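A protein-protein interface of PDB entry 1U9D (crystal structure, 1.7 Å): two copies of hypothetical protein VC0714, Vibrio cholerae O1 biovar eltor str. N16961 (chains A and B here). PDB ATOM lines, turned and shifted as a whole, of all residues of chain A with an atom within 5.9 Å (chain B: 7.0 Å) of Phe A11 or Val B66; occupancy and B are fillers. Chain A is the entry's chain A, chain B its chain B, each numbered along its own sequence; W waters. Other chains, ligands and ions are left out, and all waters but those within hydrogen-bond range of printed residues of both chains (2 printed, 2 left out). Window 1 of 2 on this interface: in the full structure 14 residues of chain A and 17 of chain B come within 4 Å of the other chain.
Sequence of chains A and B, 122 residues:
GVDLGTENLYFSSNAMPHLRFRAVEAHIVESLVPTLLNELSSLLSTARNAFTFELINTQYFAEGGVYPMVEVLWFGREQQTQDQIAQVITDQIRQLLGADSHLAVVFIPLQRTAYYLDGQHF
The backbone carbonyl oxygen of Tyr A10 is in hydrogen-bond range of the backbone NH of Val B66 (2.9 Å).
N of Ser A12 lies within hydrogen-bond range of O of Val B66, 2.9 Å away.
The side-chain hydroxyl (OG) of Ser A12 lies close to the side-chain hydroxyl (OH) of Tyr B67.
The backbone NH (N) of Asn A8 lies within hydrogen-bond range of the side-chain amide oxygen (OE1) of Gln B59, at 3.3 Å.
The side-chain hydroxyl of Tyr B60 is in hydrogen-bond range of the backbone NH of Ala B23.
The backbone carbonyl oxygen (O) of Asn A14 sits at hydrogen-bond distance from the guanidinium group (NH2) of Arg A112 (3.1 Å).
The side-chain hydroxyl of Thr B58 sits at hydrogen-bond distance from the side-chain hydroxyl of Tyr B60 (2.6 Å).
The backbone carbonyl oxygen of Phe A11 sits at hydrogen-bond distance from the guanidinium group of Arg A112.
ND2 of Asn A8 touches CG of Glu B25 (3.8 Å).
Tyr A10 touches Tyr B60.
CG of Tyr A10 touches CD1 of Phe B61, at 3.8 Å.
Gly B65 touches Tyr A10.
Phe A11 touches Ala B23.
CZ of Phe A11 touches N of Val B24, at 3.7 Å.
CA of Phe A11 touches O of Val B66 (3.7 Å).
O of Gly B64 touches OG of Ser A12, at 3.8 Å.
Gly B64 touches Arg A112.
CD of Arg A112 touches N of Gly B65 (3.7 Å).
Leu A9 touches none of the printed residues of chain B.
Of the printed residues of chain B, Phe A11 touches Ala B23 (3.4 Å), Val B24 (3.7 Å), Glu B25 (3.7 Å) and Val B66 (3.7 Å).
Printed residues of chain A within 4 Å of Ala B23: Phe A11.
Printed residues of chain A within 4 Å of Gln B59: Asn A8 (3.3 Å).
Of the printed residues of chain A, Tyr B60 touches Tyr A10.
Of the printed residues of chain A, Phe B61 touches Tyr A10.
Ala B62 touches none of the printed residues of chain A.
Val B66 touches three residues of chain A.
The nearest residue of chain A that does not touch Val B66 is Ser A13 (4.9 Å).
Of the 9 printed residues of chain A, 5 touch a printed residue of chain B.
Hydrophobic or aromatic side chains of chain A within 4 Å of the printed part of chain B: Tyr A10 and Phe A11.
Of the 17 printed residues of chain B, 10 touch a printed residue of chain A.
Printed residues of chain B that touch a printed residue of chain A: Ala B23, Val B24, Glu B25, Gln B59, Tyr B60, Phe B61, Gly B64, Gly B65, Val B66 and Tyr B67.
Among the printed residues, 15 pairs touch across the chains.
No position is printed for both chains.
Water W2 lies within hydrogen-bond range of ND2 of Asn A8 and N of Ala B26.
Water W1 lies within hydrogen-bond range of O of Ala B62 (3.0 Å), NH1 of Arg A112 (3.3 Å) and N of Gly B65 (3.4 Å).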
ATOM      1  N   ASN A   8      17.133 -14.286   4.002  1.00  0.00           N
ATOM      2  CA  ASN A   8      15.873 -14.757   3.449  1.00  0.00           C
ATOM      3  C   ASN A   8      15.821 -14.784   1.913  1.00  0.00           C
ATOM      4  O   ASN A   8      14.755 -14.857   1.325  1.00  0.00           O
ATOM      5  CB  ASN A   8      14.705 -13.947   4.007  1.00  0.00           C
ATOM      6  CG  ASN A   8      14.712 -13.841   5.531  1.00  0.00           C
ATOM      7  OD1 ASN A   8      15.445 -14.548   6.222  1.00  0.00           O
ATOM      8  ND2 ASN A   8      13.895 -12.928   6.053  1.00  0.00           N
ATOM      9  N   LEU A   9      16.976 -14.809   1.271  1.00  0.00           N
ATOM     10  CA  LEU A   9      17.058 -14.643  -0.193  1.00  0.00           C
ATOM     11  C   LEU A   9      16.283 -15.718  -0.971  1.00  0.00           C
ATOM     12  O   LEU A   9      15.561 -15.421  -1.945  1.00  0.00           O
ATOM     13  CB  LEU A   9      18.526 -14.667  -0.627  1.00  0.00           C
ATOM     14  CG  LEU A   9      18.836 -14.513  -2.122  1.00  0.00           C
ATOM     15  CD1 LEU A   9      18.237 -13.211  -2.626  1.00  0.00           C
ATOM     16  CD2 LEU A   9      20.366 -14.539  -2.386  1.00  0.00           C
ATOM     17  N   TYR A  10      16.404 -16.975  -0.535  1.00  0.00           N
ATOM     18  CA  TYR A  10      15.828 -18.097  -1.298  1.00  0.00           C
ATOM     19  C   TYR A  10      14.420 -18.532  -0.874  1.00  0.00           C
ATOM     20  O   TYR A  10      13.878 -19.511  -1.392  1.00  0.00           O
ATOM     21  CB  TYR A  10      16.795 -19.263  -1.228  1.00  0.00           C
ATOM     22  CG  TYR A  10      18.125 -18.917  -1.838  1.00  0.00           C
ATOM     23  CD1 TYR A  10      19.262 -18.763  -1.068  1.00  0.00           C
ATOM     24  CD2 TYR A  10      18.245 -18.775  -3.222  1.00  0.00           C
ATOM     25  CE1 TYR A  10      20.477 -18.469  -1.638  1.00  0.00           C
ATOM     26  CE2 TYR A  10      19.448 -18.470  -3.792  1.00  0.00           C
ATOM     27  CZ  TYR A  10      20.565 -18.322  -3.004  1.00  0.00           C
ATOM     28  OH  TYR A  10      21.767 -18.052  -3.587  1.00  0.00           O
ATOM     29  N   PHE A  11      13.807 -17.791   0.033  1.00  0.00           N
ATOM     30  CA  PHE A  11      12.427 -18.073   0.412  1.00  0.00           C
ATOM     31  C   PHE A  11      11.520 -18.088  -0.820  1.00  0.00           C
ATOM     32  O   PHE A  11      11.611 -17.218  -1.699  1.00  0.00           O
ATOM     33  CB  PHE A  11      11.883 -16.995   1.338  1.00  0.00           C
ATOM     34  CG  PHE A  11      12.402 -17.036   2.751  1.00  0.00           C
ATOM     35  CD1 PHE A  11      13.482 -17.815   3.130  1.00  0.00           C
ATOM     36  CD2 PHE A  11      11.787 -16.229   3.705  1.00  0.00           C
ATOM     37  CE1 PHE A  11      13.930 -17.815   4.466  1.00  0.00           C
ATOM     38  CE2 PHE A  11      12.229 -16.217   5.010  1.00  0.00           C
ATOM     39  CZ  PHE A  11      13.302 -17.007   5.396  1.00  0.00           C
ATOM     40  N   SER A  12      10.579 -19.020  -0.829  1.00  0.00           N
ATOM     41  CA  SER A  12       9.602 -19.154  -1.924  1.00  0.00           C
ATOM     42  C   SER A  12       8.720 -17.902  -1.991  1.00  0.00           C
ATOM     43  O   SER A  12       8.272 -17.459  -3.071  1.00  0.00           O
ATOM     44  CB  SER A  12       8.808 -20.451  -1.706  1.00  0.00           C
ATOM     45  OG  SER A  12       8.330 -21.001  -2.918  1.00  0.00           O
ATOM     46  N   SER A  13       8.536 -17.276  -0.832  1.00  0.00           N
ATOM     47  CA  SER A  13       7.741 -16.062  -0.725  1.00  0.00           C
ATOM     48  C   SER A  13       8.461 -14.870  -1.379  1.00  0.00           C
ATOM     49  O   SER A  13       7.817 -13.872  -1.751  1.00  0.00           O
ATOM     50  CB  SER A  13       7.410 -15.784   0.749  1.00  0.00           C
ATOM     51  OG  SER A  13       8.588 -15.601   1.523  1.00  0.00           O
ATOM     52  N   ASN A  14       9.786 -14.952  -1.510  1.00  0.00           N
ATOM     53  CA  ASN A  14      10.569 -13.895  -2.155  1.00  0.00           C
ATOM     54  C   ASN A  14      10.570 -14.128  -3.652  1.00  0.00           C
ATOM     55  O   ASN A  14      11.423 -14.859  -4.187  1.00  0.00           O
ATOM     56  CB  ASN A  14      12.018 -13.868  -1.675  1.00  0.00           C
ATOM     57  CG  ASN A  14      12.852 -12.769  -2.378  1.00  0.00           C
ATOM     58  OD1 ASN A  14      12.314 -11.924  -3.118  1.00  0.00           O
ATOM     59  ND2 ASN A  14      14.163 -12.795  -2.170  1.00  0.00           N
ATOM     60  N   ALA A  15       9.604 -13.516  -4.315  1.00  0.00           N
ATOM     61  CA  ALA A  15       9.477 -13.678  -5.754  1.00  0.00           C
ATOM     62  C   ALA A  15      10.434 -12.797  -6.578  1.00  0.00           C
ATOM     63  O   ALA A  15      10.427 -12.878  -7.796  1.00  0.00           O
ATOM     64  CB  ALA A  15       8.052 -13.420  -6.167  1.00  0.00           C
ATOM     65  N   ARG A 112      13.150 -20.175 -11.486  1.00  0.00           N
ATOM     66  CA  ARG A 112      14.267 -20.052 -10.570  1.00  0.00           C
ATOM     67  C   ARG A 112      15.533 -20.732 -11.062  1.00  0.00           C
ATOM     68  O   ARG A 112      16.610 -20.242 -10.777  1.00  0.00           O
ATOM     69  CB  ARG A 112      13.900 -20.637  -9.208  1.00  0.00           C
ATOM     70  CG  ARG A 112      12.966 -19.793  -8.404  1.00  0.00           C
ATOM     71  CD  ARG A 112      12.430 -20.530  -7.138  1.00  0.00           C
ATOM     72  NE  ARG A 112      11.606 -19.593  -6.378  1.00  0.00           N
ATOM     73  CZ  ARG A 112      12.071 -18.742  -5.475  1.00  0.00           C
ATOM     74  NH1 ARG A 112      13.356 -18.730  -5.132  1.00  0.00           N
ATOM     75  NH2 ARG A 112      11.238 -17.905  -4.891  1.00  0.00           N
ATOM     76  N   ARG B  22      11.220 -21.736  11.267  1.00  0.00           N
ATOM     77  CA  ARG B  22      12.361 -21.747  10.377  1.00  0.00           C
ATOM     78  C   ARG B  22      11.918 -21.268   9.007  1.00  0.00           C
ATOM     79  O   ARG B  22      10.814 -21.598   8.577  1.00  0.00           O
ATOM     80  CB  ARG B  22      12.858 -23.165  10.160  1.00  0.00           C
ATOM     81  CG  ARG B  22      13.184 -23.935  11.362  1.00  0.00           C
ATOM     82  CD  ARG B  22      14.069 -25.109  11.035  1.00  0.00           C
ATOM     83  NE  ARG B  22      14.511 -25.599  12.295  1.00  0.00           N
ATOM     84  CZ  ARG B  22      15.722 -25.478  12.780  1.00  0.00           C
ATOM     85  NH1 ARG B  22      16.703 -24.945  12.079  1.00  0.00           N
ATOM     86  NH2 ARG B  22      15.954 -25.953  13.982  1.00  0.00           N
ATOM     87  N   ALA B  23      12.796 -20.553   8.314  1.00  0.00           N
ATOM     88  CA  ALA B  23      12.540 -20.065   6.946  1.00  0.00           C
ATOM     89  C   ALA B  23      11.255 -19.265   6.852  1.00  0.00           C
ATOM     90  O   ALA B  23      10.505 -19.383   5.890  1.00  0.00           O
ATOM     91  CB  ALA B  23      12.539 -21.237   5.944  1.00  0.00           C
ATOM     92  N   VAL B  24      11.005 -18.438   7.862  1.00  0.00           N
ATOM     93  CA  VAL B  24       9.849 -17.562   7.917  1.00  0.00           C
ATOM     94  C   VAL B  24      10.365 -16.168   8.292  1.00  0.00           C
ATOM     95  O   VAL B  24      11.225 -16.017   9.151  1.00  0.00           O
ATOM     96  CB  VAL B  24       8.799 -18.004   8.957  1.00  0.00           C
ATOM     97  CG1 VAL B  24       8.053 -19.210   8.505  1.00  0.00           C
ATOM     98  CG2 VAL B  24       9.453 -18.304  10.279  1.00  0.00           C
ATOM     99  N   GLU B  25       9.846 -15.143   7.638  1.00  0.00           N
ATOM    100  CA  GLU B  25      10.317 -13.797   7.880  1.00  0.00           C
ATOM    101  C   GLU B  25       9.959 -13.374   9.300  1.00  0.00           C
ATOM    102  O   GLU B  25       8.897 -13.720   9.798  1.00  0.00           O
ATOM    103  CB  GLU B  25       9.698 -12.856   6.855  1.00  0.00           C
ATOM    104  CG  GLU B  25      10.435 -11.545   6.711  1.00  0.00           C
ATOM    105  CD  GLU B  25       9.776 -10.437   7.495  1.00  0.00           C
ATOM    106  OE1 GLU B  25      10.487  -9.517   7.980  1.00  0.00           O
ATOM    107  OE2 GLU B  25       8.537 -10.505   7.636  1.00  0.00           O
ATOM    108  N   ALA B  26      10.853 -12.626   9.934  1.00  0.00           N
ATOM    109  CA  ALA B  26      10.714 -12.250  11.335  1.00  0.00           C
ATOM    110  C   ALA B  26       9.409 -11.522  11.633  1.00  0.00           C
ATOM    111  O   ALA B  26       8.793 -11.760  12.670  1.00  0.00           O
ATOM    112  CB  ALA B  26      11.892 -11.371  11.756  1.00  0.00           C
ATOM    113  N   THR B  58      18.719 -18.756  10.804  1.00  0.00           N
ATOM    114  CA  THR B  58      19.650 -19.408   9.912  1.00  0.00           C
ATOM    115  C   THR B  58      19.342 -19.038   8.474  1.00  0.00           C
ATOM    116  O   THR B  58      18.358 -18.366   8.199  1.00  0.00           O
ATOM    117  CB  THR B  58      19.531 -20.912  10.089  1.00  0.00           C
ATOM    118  OG1 THR B  58      18.174 -21.317   9.880  1.00  0.00           O
ATOM    119  CG2 THR B  58      19.834 -21.304  11.546  1.00  0.00           C
ATOM    120  N   GLN B  59      20.208 -19.477   7.568  1.00  0.00           N
ATOM    121  CA  GLN B  59      20.018 -19.233   6.146  1.00  0.00           C
ATOM    122  C   GLN B  59      19.834 -20.553   5.420  1.00  0.00           C
ATOM    123  O   GLN B  59      20.549 -21.507   5.668  1.00  0.00           O
ATOM    124  CB  GLN B  59      21.195 -18.467   5.568  1.00  0.00           C
ATOM    125  CG  GLN B  59      21.453 -17.110   6.270  1.00  0.00           C
ATOM    126  CD  GLN B  59      20.202 -16.248   6.427  1.00  0.00           C
ATOM    127  OE1 GLN B  59      19.368 -16.174   5.518  1.00  0.00           O
ATOM    128  NE2 GLN B  59      20.072 -15.585   7.585  1.00  0.00           N
ATOM    129  N   TYR B  60      18.879 -20.556   4.500  1.00  0.00           N
ATOM    130  CA  TYR B  60      18.369 -21.755   3.860  1.00  0.00           C
ATOM    131  C   TYR B  60      18.525 -21.624   2.355  1.00  0.00           C
ATOM    132  O   TYR B  60      18.429 -20.506   1.802  1.00  0.00           O
ATOM    133  CB  TYR B  60      16.879 -21.932   4.177  1.00  0.00           C
ATOM    134  CG  TYR B  60      16.526 -21.820   5.636  1.00  0.00           C
ATOM    135  CD1 TYR B  60      16.187 -22.928   6.383  1.00  0.00           C
ATOM    136  CD2 TYR B  60      16.528 -20.583   6.259  1.00  0.00           C
ATOM    137  CE1 TYR B  60      15.860 -22.808   7.732  1.00  0.00           C
ATOM    138  CE2 TYR B  60      16.207 -20.446   7.580  1.00  0.00           C
ATOM    139  CZ  TYR B  60      15.871 -21.556   8.320  1.00  0.00           C
ATOM    140  OH  TYR B  60      15.558 -21.341   9.649  1.00  0.00           O
ATOM    141  N   PHE B  61      18.775 -22.752   1.717  1.00  0.00           N
ATOM    142  CA  PHE B  61      18.713 -22.893   0.270  1.00  0.00           C
ATOM    143  C   PHE B  61      17.900 -24.133  -0.080  1.00  0.00           C
ATOM    144  O   PHE B  61      17.996 -25.175   0.595  1.00  0.00           O
ATOM    145  CB  PHE B  61      20.106 -23.023  -0.353  1.00  0.00           C
ATOM    146  CG  PHE B  61      20.059 -23.222  -1.843  1.00  0.00           C
ATOM    147  CD1 PHE B  61      19.892 -22.139  -2.692  1.00  0.00           C
ATOM    148  CD2 PHE B  61      20.077 -24.486  -2.384  1.00  0.00           C
ATOM    149  CE1 PHE B  61      19.799 -22.307  -4.072  1.00  0.00           C
ATOM    150  CE2 PHE B  61      19.973 -24.669  -3.762  1.00  0.00           C
ATOM    151  CZ  PHE B  61      19.848 -23.584  -4.612  1.00  0.00           C
ATOM    152  N   ALA B  62      17.072 -24.023  -1.124  1.00  0.00           N
ATOM    153  CA  ALA B  62      16.413 -25.172  -1.735  1.00  0.00           C
ATOM    154  C   ALA B  62      16.137 -24.805  -3.184  1.00  0.00           C
ATOM    155  O   ALA B  62      15.796 -23.673  -3.454  1.00  0.00           O
ATOM    156  CB  ALA B  62      15.116 -25.518  -1.053  1.00  0.00           C
ATOM    157  N   GLU B  63      16.295 -25.758  -4.091  1.00  0.00           N
ATOM    158  CA  GLU B  63      15.944 -25.529  -5.480  1.00  0.00           C
ATOM    159  C   GLU B  63      14.423 -25.435  -5.508  1.00  0.00           C
ATOM    160  O   GLU B  63      13.728 -26.252  -4.923  1.00  0.00           O
ATOM    161  CB  GLU B  63      16.482 -26.671  -6.352  1.00  0.00           C
ATOM    162  CG  GLU B  63      16.069 -26.621  -7.827  1.00  0.00           C
ATOM    163  CD  GLU B  63      17.128 -27.204  -8.754  1.00  0.00           C
ATOM    164  OE1 GLU B  63      18.331 -26.933  -8.530  1.00  0.00           O
ATOM    165  OE2 GLU B  63      16.761 -27.928  -9.716  1.00  0.00           O
ATOM    166  N   GLY B  64      13.909 -24.366  -6.100  1.00  0.00           N
ATOM    167  CA  GLY B  64      12.478 -24.162  -6.210  1.00  0.00           C
ATOM    168  C   GLY B  64      11.927 -23.242  -5.134  1.00  0.00           C
ATOM    169  O   GLY B  64      10.741 -22.922  -5.134  1.00  0.00           O
ATOM    170  N   GLY B  65      12.797 -22.816  -4.228  1.00  0.00           N
ATOM    171  CA  GLY B  65      12.464 -21.921  -3.148  1.00  0.00           C
ATOM    172  C   GLY B  65      12.265 -22.689  -1.849  1.00  0.00           C
ATOM    173  O   GLY B  65      11.869 -23.861  -1.860  1.00  0.00           O
ATOM    174  N   VAL B  66      12.567 -22.029  -0.745  1.00  0.00           N
ATOM    175  CA  VAL B  66      12.521 -22.621   0.573  1.00  0.00           C
ATOM    176  C   VAL B  66      11.124 -22.351   1.134  1.00  0.00           C
ATOM    177  O   VAL B  66      10.632 -21.223   1.080  1.00  0.00           O
ATOM    178  CB  VAL B  66      13.551 -21.986   1.530  1.00  0.00           C
ATOM    179  CG1 VAL B  66      13.475 -22.678   2.876  1.00  0.00           C
ATOM    180  CG2 VAL B  66      14.961 -22.070   0.936  1.00  0.00           C
ATOM    181  N   TYR B  67      10.493 -23.388   1.663  1.00  0.00           N
ATOM    182  CA  TYR B  67       9.160 -23.236   2.217  1.00  0.00           C
ATOM    183  C   TYR B  67       9.265 -23.101   3.737  1.00  0.00           C
ATOM    184  O   TYR B  67      10.166 -23.668   4.350  1.00  0.00           O
ATOM    185  CB  TYR B  67       8.294 -24.418   1.808  1.00  0.00           C
ATOM    186  CG  TYR B  67       7.969 -24.381   0.322  1.00  0.00           C
ATOM    187  CD1 TYR B  67       6.984 -23.531  -0.162  1.00  0.00           C
ATOM    188  CD2 TYR B  67       8.693 -25.134  -0.593  1.00  0.00           C
ATOM    189  CE1 TYR B  67       6.686 -23.462  -1.507  1.00  0.00           C
ATOM    190  CE2 TYR B  67       8.403 -25.068  -1.968  1.00  0.00           C
ATOM    191  CZ  TYR B  67       7.398 -24.223  -2.406  1.00  0.00           C
ATOM    192  OH  TYR B  67       7.074 -24.117  -3.737  1.00  0.00           O
ATOM    193  N   PRO B  68       8.362 -22.361   4.350  1.00  0.00           N
ATOM    194  CA  PRO B  68       8.441 -22.189   5.804  1.00  0.00           C
ATOM    195  C   PRO B  68       8.195 -23.483   6.552  1.00  0.00           C
ATOM    196  O   PRO B  68       7.495 -24.367   6.056  1.00  0.00           O
ATOM    197  CB  PRO B  68       7.382 -21.138   6.069  1.00  0.00           C
ATOM    198  CG  PRO B  68       6.451 -21.245   4.983  1.00  0.00           C
ATOM    199  CD  PRO B  68       7.180 -21.687   3.774  1.00  0.00           C
ATOM    200  N   MET B  69       8.791 -23.624   7.735  1.00  0.00           N
ATOM    201  CA  MET B  69       8.609 -24.822   8.521  1.00  0.00           C
ATOM    202  C   MET B  69       8.497 -24.476   9.993  1.00  0.00           C
ATOM    203  O   MET B  69       9.250 -23.639  10.486  1.00  0.00           O
ATOM    204  CB  MET B  69       9.755 -25.783   8.366  1.00  0.00           C
ATOM    205  CG  MET B  69       9.636 -26.969   9.347  1.00  0.00           C
ATOM    206  SD  MET B  69      11.143 -28.135   9.287  1.00  0.00           S
ATOM    207  CE  MET B  69      10.561 -29.235   7.733  1.00  0.00           C
HETATM  208  O   HOH W   1      15.591 -21.095  -4.984  1.00  0.00           O
HETATM  209  O   HOH W   2      13.414 -12.028   8.711  1.00  0.00           O
